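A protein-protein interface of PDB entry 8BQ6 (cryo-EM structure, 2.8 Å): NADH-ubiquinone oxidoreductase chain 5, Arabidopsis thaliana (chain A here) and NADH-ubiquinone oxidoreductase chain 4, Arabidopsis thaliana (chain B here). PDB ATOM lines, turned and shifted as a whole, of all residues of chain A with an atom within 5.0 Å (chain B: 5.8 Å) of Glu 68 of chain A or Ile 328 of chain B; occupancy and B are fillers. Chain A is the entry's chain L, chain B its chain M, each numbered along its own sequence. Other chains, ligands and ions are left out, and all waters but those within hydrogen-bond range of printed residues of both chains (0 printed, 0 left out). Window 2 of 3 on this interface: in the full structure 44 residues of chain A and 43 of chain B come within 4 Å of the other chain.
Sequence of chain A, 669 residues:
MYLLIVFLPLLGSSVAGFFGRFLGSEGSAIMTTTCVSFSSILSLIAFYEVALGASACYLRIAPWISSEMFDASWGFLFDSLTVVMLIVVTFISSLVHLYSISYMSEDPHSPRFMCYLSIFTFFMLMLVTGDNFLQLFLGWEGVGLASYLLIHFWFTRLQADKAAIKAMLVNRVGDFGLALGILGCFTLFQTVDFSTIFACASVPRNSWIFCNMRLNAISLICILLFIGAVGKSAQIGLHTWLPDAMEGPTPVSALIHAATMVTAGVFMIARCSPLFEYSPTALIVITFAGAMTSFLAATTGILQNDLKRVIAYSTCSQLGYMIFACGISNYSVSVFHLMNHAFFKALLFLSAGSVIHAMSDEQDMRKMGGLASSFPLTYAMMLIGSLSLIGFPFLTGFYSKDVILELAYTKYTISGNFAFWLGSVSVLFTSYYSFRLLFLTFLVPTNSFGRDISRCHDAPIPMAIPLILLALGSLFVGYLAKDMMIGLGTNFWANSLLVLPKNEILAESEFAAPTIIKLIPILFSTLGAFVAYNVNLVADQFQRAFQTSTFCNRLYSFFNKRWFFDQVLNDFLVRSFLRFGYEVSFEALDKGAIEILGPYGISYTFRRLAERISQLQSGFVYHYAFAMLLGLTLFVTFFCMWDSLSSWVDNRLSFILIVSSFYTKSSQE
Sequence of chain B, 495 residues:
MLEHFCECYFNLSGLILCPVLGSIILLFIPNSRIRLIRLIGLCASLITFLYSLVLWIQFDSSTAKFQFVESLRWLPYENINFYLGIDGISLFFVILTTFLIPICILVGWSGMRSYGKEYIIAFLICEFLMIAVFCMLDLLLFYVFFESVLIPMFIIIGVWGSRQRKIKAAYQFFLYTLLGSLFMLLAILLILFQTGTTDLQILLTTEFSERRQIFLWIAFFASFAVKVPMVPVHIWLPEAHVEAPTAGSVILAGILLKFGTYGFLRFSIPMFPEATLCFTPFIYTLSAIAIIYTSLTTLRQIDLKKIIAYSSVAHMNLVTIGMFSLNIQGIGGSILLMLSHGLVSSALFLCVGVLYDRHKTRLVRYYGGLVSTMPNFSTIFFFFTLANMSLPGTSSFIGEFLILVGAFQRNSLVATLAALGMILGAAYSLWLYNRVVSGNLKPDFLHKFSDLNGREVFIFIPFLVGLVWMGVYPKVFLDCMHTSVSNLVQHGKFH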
ATOM      1  N   SER A  66       1.368 -21.426  -7.254  1.00  0.00           N
ATOM      2  CA  SER A  66       1.075 -22.519  -6.339  1.00  0.00           C
ATOM      3  C   SER A  66       0.781 -21.922  -4.970  1.00  0.00           C
ATOM      4  O   SER A  66       1.704 -21.616  -4.209  1.00  0.00           O
ATOM      5  CB  SER A  66       2.243 -23.499  -6.278  1.00  0.00           C
ATOM      6  OG  SER A  66       1.793 -24.808  -5.985  1.00  0.00           O
ATOM      7  N   SER A  67      -0.502 -21.756  -4.662  1.00  0.00           N
ATOM      8  CA  SER A  67      -0.929 -21.202  -3.379  1.00  0.00           C
ATOM      9  C   SER A  67      -1.997 -22.126  -2.803  1.00  0.00           C
ATOM     10  O   SER A  67      -3.166 -22.042  -3.193  1.00  0.00           O
ATOM     11  CB  SER A  67      -1.454 -19.782  -3.541  1.00  0.00           C
ATOM     12  OG  SER A  67      -1.734 -19.203  -2.282  1.00  0.00           O
ATOM     13  N   GLU A  68      -1.595 -22.995  -1.878  1.00  0.00           N
ATOM     14  CA  GLU A  68      -2.499 -23.968  -1.246  1.00  0.00           C
ATOM     15  C   GLU A  68      -3.063 -24.857  -2.355  1.00  0.00           C
ATOM     16  O   GLU A  68      -2.283 -25.536  -3.042  1.00  0.00           O
ATOM     17  CB  GLU A  68      -3.526 -23.228  -0.395  1.00  0.00           C
ATOM     18  CG  GLU A  68      -4.348 -24.132   0.498  1.00  0.00           C
ATOM     19  CD  GLU A  68      -5.786 -23.675   0.605  1.00  0.00           C
ATOM     20  OE1 GLU A  68      -6.527 -23.849  -0.384  1.00  0.00           O
ATOM     21  OE2 GLU A  68      -6.189 -23.177   1.675  1.00  0.00           O
ATOM     22  N   MET A  69      -4.381 -24.896  -2.571  1.00  0.00           N
ATOM     23  CA  MET A  69      -4.919 -25.761  -3.616  1.00  0.00           C
ATOM     24  C   MET A  69      -4.809 -25.126  -4.998  1.00  0.00           C
ATOM     25  O   MET A  69      -4.914 -25.834  -6.006  1.00  0.00           O
ATOM     26  CB  MET A  69      -6.372 -26.118  -3.309  1.00  0.00           C
ATOM     27  CG  MET A  69      -6.553 -26.995  -2.077  1.00  0.00           C
ATOM     28  SD  MET A  69      -5.921 -28.669  -2.286  1.00  0.00           S
ATOM     29  CE  MET A  69      -7.319 -29.444  -3.083  1.00  0.00           C
ATOM     30  N   PHE A  70      -4.590 -23.806  -5.053  1.00  0.00           N
ATOM     31  CA  PHE A  70      -4.406 -23.100  -6.350  1.00  0.00           C
ATOM     32  C   PHE A  70      -3.141 -23.654  -6.994  1.00  0.00           C
ATOM     33  O   PHE A  70      -2.081 -23.590  -6.359  1.00  0.00           O
ATOM     34  CB  PHE A  70      -4.402 -21.583  -6.160  1.00  0.00           C
ATOM     35  CG  PHE A  70      -4.815 -20.818  -7.388  1.00  0.00           C
ATOM     36  CD1 PHE A  70      -3.890 -20.089  -8.115  1.00  0.00           C
ATOM     37  CD2 PHE A  70      -6.128 -20.846  -7.825  1.00  0.00           C
ATOM     38  CE1 PHE A  70      -4.273 -19.390  -9.248  1.00  0.00           C
ATOM     39  CE2 PHE A  70      -6.510 -20.152  -8.960  1.00  0.00           C
ATOM     40  CZ  PHE A  70      -5.582 -19.424  -9.665  1.00  0.00           C
ATOM     41  N   GLN A 190     -11.749 -27.040  -6.689  1.00  0.00           N
ATOM     42  CA  GLN A 190     -10.477 -26.829  -5.996  1.00  0.00           C
ATOM     43  C   GLN A 190      -9.277 -27.081  -6.905  1.00  0.00           C
ATOM     44  O   GLN A 190      -8.242 -27.579  -6.459  1.00  0.00           O
ATOM     45  CB  GLN A 190     -10.394 -27.679  -4.726  1.00  0.00           C
ATOM     46  CG  GLN A 190     -11.373 -27.229  -3.654  1.00  0.00           C
ATOM     47  CD  GLN A 190     -11.048 -25.848  -3.124  1.00  0.00           C
ATOM     48  OE1 GLN A 190     -10.053 -25.659  -2.425  1.00  0.00           O
ATOM     49  NE2 GLN A 190     -11.883 -24.872  -3.460  1.00  0.00           N
ATOM     50  N   LEU B 326      -9.162 -13.352   4.458  1.00  0.00           N
ATOM     51  CA  LEU B 326      -8.710 -14.217   5.550  1.00  0.00           C
ATOM     52  C   LEU B 326      -8.507 -15.664   5.102  1.00  0.00           C
ATOM     53  O   LEU B 326      -8.938 -16.607   5.766  1.00  0.00           O
ATOM     54  CB  LEU B 326      -9.671 -14.157   6.739  1.00  0.00           C
ATOM     55  CG  LEU B 326      -9.313 -13.188   7.863  1.00  0.00           C
ATOM     56  CD1 LEU B 326      -7.913 -13.468   8.369  1.00  0.00           C
ATOM     57  CD2 LEU B 326      -9.444 -11.756   7.405  1.00  0.00           C
ATOM     58  N   ASN B 327      -7.825 -15.841   3.974  1.00  0.00           N
ATOM     59  CA  ASN B 327      -7.438 -17.170   3.526  1.00  0.00           C
ATOM     60  C   ASN B 327      -6.079 -17.073   2.847  1.00  0.00           C
ATOM     61  O   ASN B 327      -5.509 -15.988   2.705  1.00  0.00           O
ATOM     62  CB  ASN B 327      -8.495 -17.790   2.605  1.00  0.00           C
ATOM     63  CG  ASN B 327      -9.158 -16.774   1.715  1.00  0.00           C
ATOM     64  OD1 ASN B 327      -8.656 -15.666   1.542  1.00  0.00           O
ATOM     65  ND2 ASN B 327     -10.284 -17.148   1.128  1.00  0.00           N
ATOM     66  N   ILE B 328      -5.554 -18.226   2.437  1.00  0.00           N
ATOM     67  CA  ILE B 328      -4.188 -18.284   1.925  1.00  0.00           C
ATOM     68  C   ILE B 328      -4.049 -17.453   0.658  1.00  0.00           C
ATOM     69  O   ILE B 328      -3.087 -16.693   0.498  1.00  0.00           O
ATOM     70  CB  ILE B 328      -3.771 -19.744   1.690  1.00  0.00           C
ATOM     71  CG1 ILE B 328      -4.106 -20.570   2.926  1.00  0.00           C
ATOM     72  CG2 ILE B 328      -2.293 -19.833   1.340  1.00  0.00           C
ATOM     73  CD1 ILE B 328      -3.282 -20.191   4.123  1.00  0.00           C
ATOM     74  N   GLN B 329      -5.003 -17.587  -0.261  1.00  0.00           N
ATOM     75  CA  GLN B 329      -4.921 -16.847  -1.514  1.00  0.00           C
ATOM     76  C   GLN B 329      -5.089 -15.351  -1.282  1.00  0.00           C
ATOM     77  O   GLN B 329      -4.309 -14.541  -1.795  1.00  0.00           O
ATOM     78  CB  GLN B 329      -5.964 -17.371  -2.499  1.00  0.00           C
ATOM     79  CG  GLN B 329      -5.725 -18.810  -2.928  1.00  0.00           C
ATOM     80  CD  GLN B 329      -6.380 -19.808  -2.005  1.00  0.00           C
ATOM     81  OE1 GLN B 329      -7.396 -19.514  -1.378  1.00  0.00           O
ATOM     82  NE2 GLN B 329      -5.803 -20.997  -1.915  1.00  0.00           N
ATOM     83  N   GLY B 330      -6.093 -14.967  -0.493  1.00  0.00           N
ATOM     84  CA  GLY B 330      -6.356 -13.551  -0.292  1.00  0.00           C
ATOM     85  C   GLY B 330      -5.206 -12.827   0.380  1.00  0.00           C
ATOM     86  O   GLY B 330      -4.744 -11.791  -0.102  1.00  0.00           O
ATOM     87  N   ILE B 331      -4.725 -13.363   1.505  1.00  0.00           N
ATOM     88  CA  ILE B 331      -3.615 -12.726   2.211  1.00  0.00           C
ATOM     89  C   ILE B 331      -2.314 -12.901   1.440  1.00  0.00           C
ATOM     90  O   ILE B 331      -1.487 -11.982   1.378  1.00  0.00           O
ATOM     91  CB  ILE B 331      -3.508 -13.259   3.652  1.00  0.00           C
ATOM     92  CG1 ILE B 331      -4.553 -12.583   4.534  1.00  0.00           C
ATOM     93  CG2 ILE B 331      -2.133 -12.992   4.233  1.00  0.00           C
ATOM     94  CD1 ILE B 331      -5.217 -13.509   5.494  1.00  0.00           C
ATOM     95  N   GLY B 332      -2.104 -14.074   0.844  1.00  0.00           N
ATOM     96  CA  GLY B 332      -0.935 -14.255  -0.003  1.00  0.00           C
ATOM     97  C   GLY B 332      -0.941 -13.321  -1.198  1.00  0.00           C
ATOM     98  O   GLY B 332       0.084 -12.734  -1.550  1.00  0.00           O
ATOM     99  N   GLY B 333      -2.101 -13.175  -1.840  1.00  0.00           N
ATOM    100  CA  GLY B 333      -2.203 -12.259  -2.964  1.00  0.00           C
ATOM    101  C   GLY B 333      -2.062 -10.807  -2.553  1.00  0.00           C
ATOM    102  O   GLY B 333      -1.508  -9.992  -3.297  1.00  0.00           O
ATOM    103  N   GLN B 409     -14.130 -17.033  -2.761  1.00  0.00           N
ATOM    104  CA  GLN B 409     -14.434 -18.102  -1.820  1.00  0.00           C
ATOM    105  C   GLN B 409     -15.139 -17.602  -0.568  1.00  0.00           C
ATOM    106  O   GLN B 409     -15.632 -18.421   0.214  1.00  0.00           O
ATOM    107  CB  GLN B 409     -13.158 -18.824  -1.415  1.00  0.00           C
ATOM    108  CG  GLN B 409     -12.409 -19.444  -2.554  1.00  0.00           C
ATOM    109  CD  GLN B 409     -11.235 -20.244  -2.063  1.00  0.00           C
ATOM    110  OE1 GLN B 409     -11.090 -20.485  -0.868  1.00  0.00           O
ATOM    111  NE2 GLN B 409     -10.375 -20.638  -2.977  1.00  0.00           N
ATOM    112  N   HIS B 482       4.296 -18.661   3.073  1.00  0.00           N
ATOM    113  CA  HIS B 482       3.076 -19.419   3.335  1.00  0.00           C
ATOM    114  C   HIS B 482       2.955 -19.853   4.789  1.00  0.00           C
ATOM    115  O   HIS B 482       1.842 -20.017   5.300  1.00  0.00           O
ATOM    116  CB  HIS B 482       3.004 -20.636   2.417  1.00  0.00           C
ATOM    117  CG  HIS B 482       2.376 -20.346   1.092  1.00  0.00           C
ATOM    118  ND1 HIS B 482       2.657 -21.075  -0.043  1.00  0.00           N
ATOM    119  CD2 HIS B 482       1.501 -19.385   0.715  1.00  0.00           C
ATOM    120  CE1 HIS B 482       1.967 -20.588  -1.058  1.00  0.00           C
ATOM    121  NE2 HIS B 482       1.258 -19.561  -0.625  1.00  0.00           N
ATOM    122  N   VAL B 485       1.798 -16.760   6.581  1.00  0.00           N
ATOM    123  CA  VAL B 485       0.439 -16.487   6.123  1.00  0.00           C
ATOM    124  C   VAL B 485      -0.534 -17.482   6.736  1.00  0.00           C
ATOM    125  O   VAL B 485      -1.627 -17.111   7.179  1.00  0.00           O
ATOM    126  CB  VAL B 485       0.378 -16.506   4.585  1.00  0.00           C
ATOM    127  CG1 VAL B 485      -1.062 -16.639   4.112  1.00  0.00           C
ATOM    128  CG2 VAL B 485       1.009 -15.253   4.015  1.00  0.00           C
ATOM    129  N   SER B 486      -0.149 -18.758   6.783  1.00  0.00           N
ATOM    130  CA  SER B 486      -1.048 -19.785   7.298  1.00  0.00           C
ATOM    131  C   SER B 486      -1.388 -19.539   8.759  1.00  0.00           C
ATOM    132  O   SER B 486      -2.547 -19.667   9.167  1.00  0.00           O
ATOM    133  CB  SER B 486      -0.416 -21.162   7.125  1.00  0.00           C
ATOM    134  OG  SER B 486      -0.364 -21.513   5.757  1.00  0.00           O
ATOM    135  N   VAL B 489      -3.791 -16.618   9.294  1.00  0.00           N
ATOM    136  CA  VAL B 489      -5.181 -16.945   9.004  1.00  0.00           C
ATOM    137  C   VAL B 489      -5.785 -17.745  10.150  1.00  0.00           C
ATOM    138  O   VAL B 489      -6.951 -17.557  10.517  1.00  0.00           O
ATOM    139  CB  VAL B 489      -5.257 -17.718   7.675  1.00  0.00           C
ATOM    140  CG1 VAL B 489      -6.674 -18.160   7.390  1.00  0.00           C
ATOM    141  CG2 VAL B 489      -4.682 -16.891   6.542  1.00  0.00           C
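Of the 13 printed residues of chain B, 3 touch a printed residue of chain A. Hydrophobic or aromatic side chains of chain B that line the printed part of chain A: Ile 328 and His 482. Among the printed residues, 6 pairs touch across the chains.
The side-chain hydroxyl (OG) of Ser 486 of chain B lies within hydrogen-bond range of the backbone carbonyl oxygen (O) of His 482 of chain B (2.7 Å).
His 482 of chain B touches Ser 66 of chain A (CE1 to O, 3.3 Å). Ile 328 of chain B touches Ser 67 of chain A (CG2 to OG, 3.7 Å). Ile 328 of chain B touches Glu 68 of chain A.
Printed residues of chain B within 4 Å of Ser 66 of chain A: His 482 (3.3 Å). Glu 68 of chain A touches two residues of chain B. Of chain A, only Ser 67 and Glu 68 come within 4 Å of Ile 328 of chain B. Of the printed residues of chain A, Gln 329 of chain B touches Ser 67 (3.1 Å) and Glu 68 (3.3 Å). The nearest residue of chain B that does not touch Glu 68 of chain A is His 482 of chain B (4.4 Å). The nearest printed residue of chain A that does not touch Ile 328 of chain B is Met 69 of chain A (6.7 Å).
NE2 of His 482 of chain B lies within hydrogen-bond range of OG of Ser 67 of chain A. NE2 of Gln 329 of chain B sits at hydrogen-bond distance from OE1 of Glu 68 of chain A (3.3 Å). NE2 of Gln 329 of chain B sits at hydrogen-bond distance from O of Ser 67 of chain A (3.1 Å).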
